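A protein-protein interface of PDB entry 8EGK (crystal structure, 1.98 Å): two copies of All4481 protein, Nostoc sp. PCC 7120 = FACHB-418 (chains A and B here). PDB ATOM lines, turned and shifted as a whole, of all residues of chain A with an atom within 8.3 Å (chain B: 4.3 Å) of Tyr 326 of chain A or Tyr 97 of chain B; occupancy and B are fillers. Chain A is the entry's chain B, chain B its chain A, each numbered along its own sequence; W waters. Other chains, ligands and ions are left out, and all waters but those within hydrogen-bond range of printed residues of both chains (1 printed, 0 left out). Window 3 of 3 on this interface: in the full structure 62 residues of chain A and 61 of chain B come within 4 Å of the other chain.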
ATOM      1  N   TRP A 150     -14.502   5.349 -23.374  1.00  0.00           N
ATOM      2  CA  TRP A 150     -13.916   4.023 -23.487  1.00  0.00           C
ATOM      3  C   TRP A 150     -12.395   4.078 -23.368  1.00  0.00           C
ATOM      4  O   TRP A 150     -11.789   3.221 -22.714  1.00  0.00           O
ATOM      5  CB  TRP A 150     -14.306   3.345 -24.799  1.00  0.00           C
ATOM      6  CG  TRP A 150     -13.613   2.031 -24.899  1.00  0.00           C
ATOM      7  CD1 TRP A 150     -14.003   0.855 -24.320  1.00  0.00           C
ATOM      8  CD2 TRP A 150     -12.377   1.756 -25.570  1.00  0.00           C
ATOM      9  NE1 TRP A 150     -13.092  -0.132 -24.600  1.00  0.00           N
ATOM     10  CE2 TRP A 150     -12.086   0.393 -25.369  1.00  0.00           C
ATOM     11  CE3 TRP A 150     -11.490   2.531 -26.324  1.00  0.00           C
ATOM     12  CZ2 TRP A 150     -10.950  -0.216 -25.903  1.00  0.00           C
ATOM     13  CZ3 TRP A 150     -10.365   1.934 -26.846  1.00  0.00           C
ATOM     14  CH2 TRP A 150     -10.100   0.570 -26.638  1.00  0.00           C
ATOM     15  N   ARG A 154     -10.485   1.786 -20.722  1.00  0.00           N
ATOM     16  CA  ARG A 154      -9.612   0.668 -21.040  1.00  0.00           C
ATOM     17  C   ARG A 154      -8.172   0.934 -20.624  1.00  0.00           C
ATOM     18  O   ARG A 154      -7.463  -0.005 -20.241  1.00  0.00           O
ATOM     19  CB  ARG A 154      -9.648   0.370 -22.531  1.00  0.00           C
ATOM     20  CG  ARG A 154      -8.979  -0.938 -22.917  1.00  0.00           C
ATOM     21  CD  ARG A 154      -9.681  -2.115 -22.285  1.00  0.00           C
ATOM     22  NE  ARG A 154      -9.270  -3.383 -22.874  1.00  0.00           N
ATOM     23  CZ  ARG A 154      -8.240  -4.109 -22.458  1.00  0.00           C
ATOM     24  NH1 ARG A 154      -7.491  -3.725 -21.435  1.00  0.00           N
ATOM     25  NH2 ARG A 154      -7.956  -5.248 -23.082  1.00  0.00           N
ATOM     26  N   PHE A 155      -7.723   2.191 -20.691  1.00  0.00           N
ATOM     27  CA  PHE A 155      -6.299   2.486 -20.580  1.00  0.00           C
ATOM     28  C   PHE A 155      -5.874   3.057 -19.235  1.00  0.00           C
ATOM     29  O   PHE A 155      -4.710   2.894 -18.860  1.00  0.00           O
ATOM     30  CB  PHE A 155      -5.868   3.444 -21.700  1.00  0.00           C
ATOM     31  CG  PHE A 155      -5.749   2.773 -23.045  1.00  0.00           C
ATOM     32  CD1 PHE A 155      -4.594   2.106 -23.398  1.00  0.00           C
ATOM     33  CD2 PHE A 155      -6.801   2.786 -23.937  1.00  0.00           C
ATOM     34  CE1 PHE A 155      -4.483   1.473 -24.616  1.00  0.00           C
ATOM     35  CE2 PHE A 155      -6.697   2.153 -25.163  1.00  0.00           C
ATOM     36  CZ  PHE A 155      -5.540   1.501 -25.505  1.00  0.00           C
ATOM     37  N   LEU A 158      -4.465   0.256 -17.303  1.00  0.00           N
ATOM     38  CA  LEU A 158      -3.227  -0.267 -17.873  1.00  0.00           C
ATOM     39  C   LEU A 158      -2.031   0.608 -17.513  1.00  0.00           C
ATOM     40  O   LEU A 158      -0.930   0.098 -17.271  1.00  0.00           O
ATOM     41  CB  LEU A 158      -3.363  -0.386 -19.389  1.00  0.00           C
ATOM     42  CG  LEU A 158      -4.488  -1.307 -19.860  1.00  0.00           C
ATOM     43  CD1 LEU A 158      -4.747  -1.103 -21.344  1.00  0.00           C
ATOM     44  CD2 LEU A 158      -4.167  -2.759 -19.567  1.00  0.00           C
ATOM     45  N   LEU A 323     -19.275  -9.712 -33.484  1.00  0.00           N
ATOM     46  CA  LEU A 323     -19.331  -9.638 -32.034  1.00  0.00           C
ATOM     47  C   LEU A 323     -18.178 -10.465 -31.486  1.00  0.00           C
ATOM     48  O   LEU A 323     -18.048 -11.649 -31.815  1.00  0.00           O
ATOM     49  CB  LEU A 323     -20.666 -10.157 -31.504  1.00  0.00           C
ATOM     50  CG  LEU A 323     -21.008  -9.678 -30.097  1.00  0.00           C
ATOM     51  CD1 LEU A 323     -21.740  -8.354 -30.145  1.00  0.00           C
ATOM     52  CD2 LEU A 323     -21.848 -10.714 -29.366  1.00  0.00           C
ATOM     53  N   THR A 324     -17.328  -9.837 -30.683  1.00  0.00           N
ATOM     54  CA  THR A 324     -16.181 -10.517 -30.109  1.00  0.00           C
ATOM     55  C   THR A 324     -15.935  -9.962 -28.715  1.00  0.00           C
ATOM     56  O   THR A 324     -16.304  -8.824 -28.408  1.00  0.00           O
ATOM     57  CB  THR A 324     -14.930 -10.341 -30.971  1.00  0.00           C
ATOM     58  OG1 THR A 324     -14.445  -8.991 -30.840  1.00  0.00           O
ATOM     59  CG2 THR A 324     -15.249 -10.629 -32.425  1.00  0.00           C
ATOM     60  N   GLN A 325     -15.319 -10.785 -27.871  1.00  0.00           N
ATOM     61  CA  GLN A 325     -14.916 -10.393 -26.527  1.00  0.00           C
ATOM     62  C   GLN A 325     -13.417 -10.650 -26.426  1.00  0.00           C
ATOM     63  O   GLN A 325     -12.985 -11.679 -25.908  1.00  0.00           O
ATOM     64  CB  GLN A 325     -15.675 -11.137 -25.472  1.00  0.00           C
ATOM     65  CG  GLN A 325     -15.229 -10.793 -24.062  1.00  0.00           C
ATOM     66  CD  GLN A 325     -16.373 -10.801 -23.068  1.00  0.00           C
ATOM     67  OE1 GLN A 325     -17.360 -11.521 -23.249  1.00  0.00           O
ATOM     68  NE2 GLN A 325     -16.241 -10.009 -22.004  1.00  0.00           N
ATOM     69  N   TYR A 326     -12.626  -9.716 -26.948  1.00  0.00           N
ATOM     70  CA  TYR A 326     -11.179  -9.825 -26.846  1.00  0.00           C
ATOM     71  C   TYR A 326     -10.684  -9.274 -25.517  1.00  0.00           C
ATOM     72  O   TYR A 326      -9.647  -9.713 -25.013  1.00  0.00           O
ATOM     73  CB  TYR A 326     -10.509  -9.081 -28.003  1.00  0.00           C
ATOM     74  CG  TYR A 326     -10.274  -9.938 -29.224  1.00  0.00           C
ATOM     75  CD1 TYR A 326      -9.290 -10.916 -29.224  1.00  0.00           C
ATOM     76  CD2 TYR A 326     -11.033  -9.772 -30.374  1.00  0.00           C
ATOM     77  CE1 TYR A 326      -9.069 -11.708 -30.335  1.00  0.00           C
ATOM     78  CE2 TYR A 326     -10.821 -10.558 -31.486  1.00  0.00           C
ATOM     79  CZ  TYR A 326      -9.837 -11.526 -31.462  1.00  0.00           C
ATOM     80  OH  TYR A 326      -9.614 -12.313 -32.572  1.00  0.00           O
ATOM     81  N   GLY A 327     -11.410  -8.320 -24.942  1.00  0.00           N
ATOM     82  CA  GLY A 327     -11.022  -7.711 -23.697  1.00  0.00           C
ATOM     83  C   GLY A 327     -12.093  -7.849 -22.634  1.00  0.00           C
ATOM     84  O   GLY A 327     -12.901  -8.780 -22.644  1.00  0.00           O
ATOM     85  N   PRO A 328     -12.114  -6.906 -21.691  1.00  0.00           N
ATOM     86  CA  PRO A 328     -13.092  -6.975 -20.596  1.00  0.00           C
ATOM     87  C   PRO A 328     -14.529  -6.711 -21.026  1.00  0.00           C
ATOM     88  O   PRO A 328     -15.445  -6.959 -20.233  1.00  0.00           O
ATOM     89  CB  PRO A 328     -12.611  -5.899 -19.619  1.00  0.00           C
ATOM     90  CG  PRO A 328     -11.509  -5.157 -20.287  1.00  0.00           C
ATOM     91  CD  PRO A 328     -11.301  -5.676 -21.658  1.00  0.00           C
ATOM     92  N   GLU A 329     -14.758  -6.223 -22.243  1.00  0.00           N
ATOM     93  CA  GLU A 329     -16.100  -5.924 -22.725  1.00  0.00           C
ATOM     94  C   GLU A 329     -16.291  -6.526 -24.110  1.00  0.00           C
ATOM     95  O   GLU A 329     -15.333  -6.772 -24.848  1.00  0.00           O
ATOM     96  CB  GLU A 329     -16.349  -4.420 -22.761  1.00  0.00           C
ATOM     97  CG  GLU A 329     -16.054  -3.734 -21.436  1.00  0.00           C
ATOM     98  CD  GLU A 329     -16.437  -2.266 -21.426  1.00  0.00           C
ATOM     99  OE1 GLU A 329     -16.134  -1.560 -22.412  1.00  0.00           O
ATOM    100  OE2 GLU A 329     -17.038  -1.819 -20.426  1.00  0.00           O
ATOM    101  N   VAL A 330     -17.558  -6.784 -24.449  1.00  0.00           N
ATOM    102  CA  VAL A 330     -17.876  -7.270 -25.782  1.00  0.00           C
ATOM    103  C   VAL A 330     -17.766  -6.119 -26.772  1.00  0.00           C
ATOM    104  O   VAL A 330     -18.155  -4.979 -26.473  1.00  0.00           O
ATOM    105  CB  VAL A 330     -19.281  -7.898 -25.806  1.00  0.00           C
ATOM    106  CG1 VAL A 330     -20.354  -6.868 -25.557  1.00  0.00           C
ATOM    107  CG2 VAL A 330     -19.533  -8.590 -27.139  1.00  0.00           C
ATOM    108  N   THR A 331     -17.233  -6.411 -27.953  1.00  0.00           N
ATOM    109  CA  THR A 331     -17.048  -5.430 -29.013  1.00  0.00           C
ATOM    110  C   THR A 331     -17.972  -5.779 -30.163  1.00  0.00           C
ATOM    111  O   THR A 331     -17.902  -6.886 -30.701  1.00  0.00           O
ATOM    112  CB  THR A 331     -15.600  -5.397 -29.498  1.00  0.00           C
ATOM    113  OG1 THR A 331     -14.705  -5.202 -28.389  1.00  0.00           O
ATOM    114  CG2 THR A 331     -15.409  -4.265 -30.511  1.00  0.00           C
ATOM    115  N   ARG A 338     -17.185   0.895 -33.810  1.00  0.00           N
ATOM    116  CA  ARG A 338     -17.085  -0.138 -32.791  1.00  0.00           C
ATOM    117  C   ARG A 338     -17.759   0.320 -31.508  1.00  0.00           C
ATOM    118  O   ARG A 338     -17.506   1.428 -31.024  1.00  0.00           O
ATOM    119  CB  ARG A 338     -15.628  -0.497 -32.521  1.00  0.00           C
ATOM    120  CG  ARG A 338     -15.075  -1.464 -33.543  1.00  0.00           C
ATOM    121  CD  ARG A 338     -13.614  -1.237 -33.739  1.00  0.00           C
ATOM    122  NE  ARG A 338     -13.017  -2.211 -34.642  1.00  0.00           N
ATOM    123  CZ  ARG A 338     -11.711  -2.442 -34.693  1.00  0.00           C
ATOM    124  NH1 ARG A 338     -10.866  -1.740 -33.967  1.00  0.00           N
ATOM    125  NH2 ARG A 338     -11.252  -3.410 -35.474  1.00  0.00           N
ATOM    126  N   ASN A 340     -18.079  -0.791 -27.634  1.00  0.00           N
ATOM    127  CA  ASN A 340     -17.650  -1.596 -26.491  1.00  0.00           C
ATOM    128  C   ASN A 340     -18.735  -1.477 -25.422  1.00  0.00           C
ATOM    129  O   ASN A 340     -18.927  -0.410 -24.840  1.00  0.00           O
ATOM    130  CB  ASN A 340     -16.292  -1.160 -25.951  1.00  0.00           C
ATOM    131  CG  ASN A 340     -15.154  -1.567 -26.861  1.00  0.00           C
ATOM    132  OD1 ASN A 340     -14.841  -2.759 -26.999  1.00  0.00           O
ATOM    133  ND2 ASN A 340     -14.507  -0.586 -27.471  1.00  0.00           N
ATOM    134  N   TRP B  77      -2.126  -0.567 -34.758  1.00  0.00           N
ATOM    135  CA  TRP B  77      -1.941  -0.897 -33.352  1.00  0.00           C
ATOM    136  C   TRP B  77      -0.878  -1.971 -33.174  1.00  0.00           C
ATOM    137  O   TRP B  77      -0.099  -1.926 -32.216  1.00  0.00           O
ATOM    138  CB  TRP B  77      -3.266  -1.355 -32.748  1.00  0.00           C
ATOM    139  CG  TRP B  77      -3.249  -1.526 -31.270  1.00  0.00           C
ATOM    140  CD1 TRP B  77      -3.502  -2.676 -30.581  1.00  0.00           C
ATOM    141  CD2 TRP B  77      -2.987  -0.517 -30.285  1.00  0.00           C
ATOM    142  NE1 TRP B  77      -3.423  -2.443 -29.231  1.00  0.00           N
ATOM    143  CE2 TRP B  77      -3.090  -1.130 -29.023  1.00  0.00           C
ATOM    144  CE3 TRP B  77      -2.668   0.837 -30.349  1.00  0.00           C
ATOM    145  CZ2 TRP B  77      -2.893  -0.434 -27.839  1.00  0.00           C
ATOM    146  CZ3 TRP B  77      -2.458   1.529 -29.172  1.00  0.00           C
ATOM    147  CH2 TRP B  77      -2.582   0.898 -27.931  1.00  0.00           C
ATOM    148  N   GLU B  95      -1.697  -5.724 -23.699  1.00  0.00           N
ATOM    149  CA  GLU B  95      -2.960  -6.387 -23.384  1.00  0.00           C
ATOM    150  C   GLU B  95      -4.054  -6.020 -24.387  1.00  0.00           C
ATOM    151  O   GLU B  95      -4.860  -6.876 -24.775  1.00  0.00           O
ATOM    152  CB  GLU B  95      -3.402  -6.011 -21.969  1.00  0.00           C
ATOM    153  CG  GLU B  95      -4.476  -6.909 -21.399  1.00  0.00           C
ATOM    154  CD  GLU B  95      -5.129  -6.323 -20.168  1.00  0.00           C
ATOM    155  OE1 GLU B  95      -4.439  -6.213 -19.130  1.00  0.00           O
ATOM    156  OE2 GLU B  95      -6.331  -5.978 -20.234  1.00  0.00           O
ATOM    157  N   VAL B  96      -4.094  -4.757 -24.821  1.00  0.00           N
ATOM    158  CA  VAL B  96      -5.238  -4.267 -25.583  1.00  0.00           C
ATOM    159  C   VAL B  96      -5.191  -4.809 -27.002  1.00  0.00           C
ATOM    160  O   VAL B  96      -4.196  -4.646 -27.717  1.00  0.00           O
ATOM    161  CB  VAL B  96      -5.264  -2.736 -25.584  1.00  0.00           C
ATOM    162  CG1 VAL B  96      -6.300  -2.235 -26.580  1.00  0.00           C
ATOM    163  CG2 VAL B  96      -5.574  -2.223 -24.201  1.00  0.00           C
ATOM    164  N   TYR B  97      -6.275  -5.458 -27.416  1.00  0.00           N
ATOM    165  CA  TYR B  97      -6.381  -5.985 -28.767  1.00  0.00           C
ATOM    166  C   TYR B  97      -6.784  -4.871 -29.726  1.00  0.00           C
ATOM    167  O   TYR B  97      -7.569  -3.984 -29.377  1.00  0.00           O
ATOM    168  CB  TYR B  97      -7.399  -7.111 -28.813  1.00  0.00           C
ATOM    169  CG  TYR B  97      -7.024  -8.309 -27.965  1.00  0.00           C
ATOM    170  CD1 TYR B  97      -6.410  -9.425 -28.531  1.00  0.00           C
ATOM    171  CD2 TYR B  97      -7.276  -8.324 -26.597  1.00  0.00           C
ATOM    172  CE1 TYR B  97      -6.074 -10.522 -27.763  1.00  0.00           C
ATOM    173  CE2 TYR B  97      -6.938  -9.421 -25.821  1.00  0.00           C
ATOM    174  CZ  TYR B  97      -6.337 -10.512 -26.408  1.00  0.00           C
ATOM    175  OH  TYR B  97      -5.997 -11.604 -25.638  1.00  0.00           O
ATOM    176  N   GLY B  98      -6.216  -4.906 -30.930  1.00  0.00           N
ATOM    177  CA  GLY B  98      -6.564  -3.917 -31.933  1.00  0.00           C
ATOM    178  C   GLY B  98      -8.023  -3.949 -32.324  1.00  0.00           C
ATOM    179  O   GLY B  98      -8.561  -2.931 -32.777  1.00  0.00           O
ATOM    180  N   GLN B  99      -8.681  -5.098 -32.144  1.00  0.00           N
ATOM    181  CA  GLN B  99     -10.091  -5.228 -32.464  1.00  0.00           C
ATOM    182  C   GLN B  99     -10.987  -4.444 -31.520  1.00  0.00           C
ATOM    183  O   GLN B  99     -12.168  -4.241 -31.841  1.00  0.00           O
ATOM    184  CB  GLN B  99     -10.474  -6.705 -32.443  1.00  0.00           C
ATOM    185  CG  GLN B  99      -9.765  -7.526 -33.511  1.00  0.00           C
ATOM    186  CD  GLN B  99      -8.523  -8.217 -32.968  1.00  0.00           C
ATOM    187  OE1 GLN B  99      -7.691  -7.592 -32.315  1.00  0.00           O
ATOM    188  NE2 GLN B  99      -8.389  -9.505 -33.252  1.00  0.00           N
ATOM    189  N   GLU B 100     -10.462  -3.988 -30.386  1.00  0.00           N
ATOM    190  CA  GLU B 100     -11.255  -3.230 -29.431  1.00  0.00           C
ATOM    191  C   GLU B 100     -11.269  -1.742 -29.729  1.00  0.00           C
ATOM    192  O   GLU B 100     -12.182  -1.037 -29.279  1.00  0.00           O
ATOM    193  CB  GLU B 100     -10.703  -3.391 -28.008  1.00  0.00           C
ATOM    194  CG  GLU B 100     -10.587  -4.790 -27.476  1.00  0.00           C
ATOM    195  CD  GLU B 100      -9.898  -4.795 -26.125  1.00  0.00           C
ATOM    196  OE1 GLU B 100     -10.495  -4.280 -25.156  1.00  0.00           O
ATOM    197  OE2 GLU B 100      -8.753  -5.290 -26.040  1.00  0.00           O
ATOM    198  N   LEU B 101     -10.233  -1.248 -30.409  1.00  0.00           N
ATOM    199  CA  LEU B 101      -9.982   0.188 -30.465  1.00  0.00           C
ATOM    200  C   LEU B 101     -11.116   0.920 -31.182  1.00  0.00           C
ATOM    201  O   LEU B 101     -11.634   0.452 -32.197  1.00  0.00           O
ATOM    202  CB  LEU B 101      -8.664   0.460 -31.180  1.00  0.00           C
ATOM    203  CG  LEU B 101      -7.372   0.012 -30.491  1.00  0.00           C
ATOM    204  CD1 LEU B 101      -6.210   0.272 -31.439  1.00  0.00           C
ATOM    205  CD2 LEU B 101      -7.175   0.749 -29.195  1.00  0.00           C
HETATM  206  O   HOH W   1     -13.933  -5.418 -33.642  1.00  0.00           O
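Of the printed residues of chain B, Trp 150 of chain A touches Glu 100 (3.7 Å) and Leu 101 (3.8 Å).
Tyr 326 of chain A touches just these residues of chain B: Tyr 97 (2.8 Å) and Gln 99 (3.1 Å).
Of the printed residues of chain B, Thr 331 of chain A touches Gln 99.
Tyr 97 of chain B touches just one residue of chain A: Tyr 326 (2.8 Å).
Gly 98 of chain B touches just one residue of chain A: Arg 338 (2.9 Å).
The nearest printed residue of chain B that does not touch Tyr 326 of chain A is Glu 100 of chain B (4.3 Å).
The nearest printed residue of chain B that does not touch Phe 155 of chain A is Leu 101 of chain B (4.1 Å).
No position is printed for both chains.
Of the 18 pairs that touch across the chains among the printed residues, none has its exchanged pair printed and touching as well.
Water W1 lies within hydrogen-bond range of O of Gln 99 of chain B and NE of Arg 338 of chain A.
The guanidinium group (NH1) of Arg 154 of chain A lies within salt-bridge range of the side-chain carboxylate (OE2) of Glu 95 of chain B (2.8 Å).
The guanidinium group (NH1) of Arg 338 of chain A lies within hydrogen-bond range of the backbone carbonyl oxygen (O) of Gly 98 of chain B.
The side-chain amide nitrogen (NE2) of Gln 99 of chain B sits close to the side-chain hydroxyl (OH) of Tyr 326 of chain A (3.1 Å).
The side-chain carboxylate of Glu 100 of chain B is in salt-bridge range of the guanidinium group of Arg 154 of chain A.
The side-chain amide nitrogen (ND2) of Asn 340 of chain A sits at hydrogen-bond distance from the backbone carbonyl oxygen (O) of Glu 100 of chain B (3.0 Å).
The backbone carbonyl oxygen (O) of Leu 101 of chain B is in hydrogen-bond range of the guanidinium group (NH1) of Arg 338 of chain A (2.9 Å).
Among the printed residues, merely in contact across the chains: Tyr 326 of chain A with Tyr 97 of chain B (2.8 Å), Leu 158 of chain A with Val 96 of chain B (3.2 Å), Arg 338 of chain A with Gln 99 of chain B (3.4 Å), Leu 158 of chain A with Glu 95 of chain B (3.5 Å), Thr 331 of chain A with Gln 99 of chain B (3.5 Å), Arg 154 of chain A with Val 96 of chain B (3.7 Å), Trp 150 of chain A with Glu 100 of chain B (3.7 Å), Gly 327 of chain A with Glu 100 of chain B (3.8 Å), Trp 150 of chain A with Leu 101 of chain B (3.8 Å), Pro 328 of chain A with Glu 100 of chain B (3.9 Å), Phe 155 of chain A with Trp 77 of chain B (3.9 Å) and Phe 155 of chain A with Val 96 of chain B (3.9 Å).
The indole nitrogen (NE1) of Trp 77 of chain B is in hydrogen-bond range of the backbone carbonyl oxygen (O) of Val 96 of chain B.
The backbone NH of Tyr 97 of chain B lies within hydrogen-bond range of the side-chain carboxylate of Glu 100 of chain B.
The indole nitrogen (NE1) of Trp 150 of chain A lies close to the side-chain amide nitrogen (ND2) of Asn 340 of chain A, 3.2 Å away.
The backbone NH (N) of Thr 331 of chain A lies within hydrogen-bond range of the backbone carbonyl oxygen (O) of Thr 324 of chain A (2.6 Å).
The side-chain hydroxyl (OG1) of Thr 331 of chain A lies within hydrogen-bond range of the side-chain amide oxygen (OD1) of Asn 340 of chain A, at 2.8 Å.
Hydrophobic or aromatic side chains of chain A that line the printed part of chain B: Trp 150, Phe 155, Leu 158, Tyr 326 and Pro 328.
Of the 8 printed residues of chain B, 8 touch a printed residue of chain A.
Hydrophobic or aromatic side chains of chain B within 4 Å of the printed part of chain A: Trp 77, Val 96, Tyr 97 and Leu 101.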
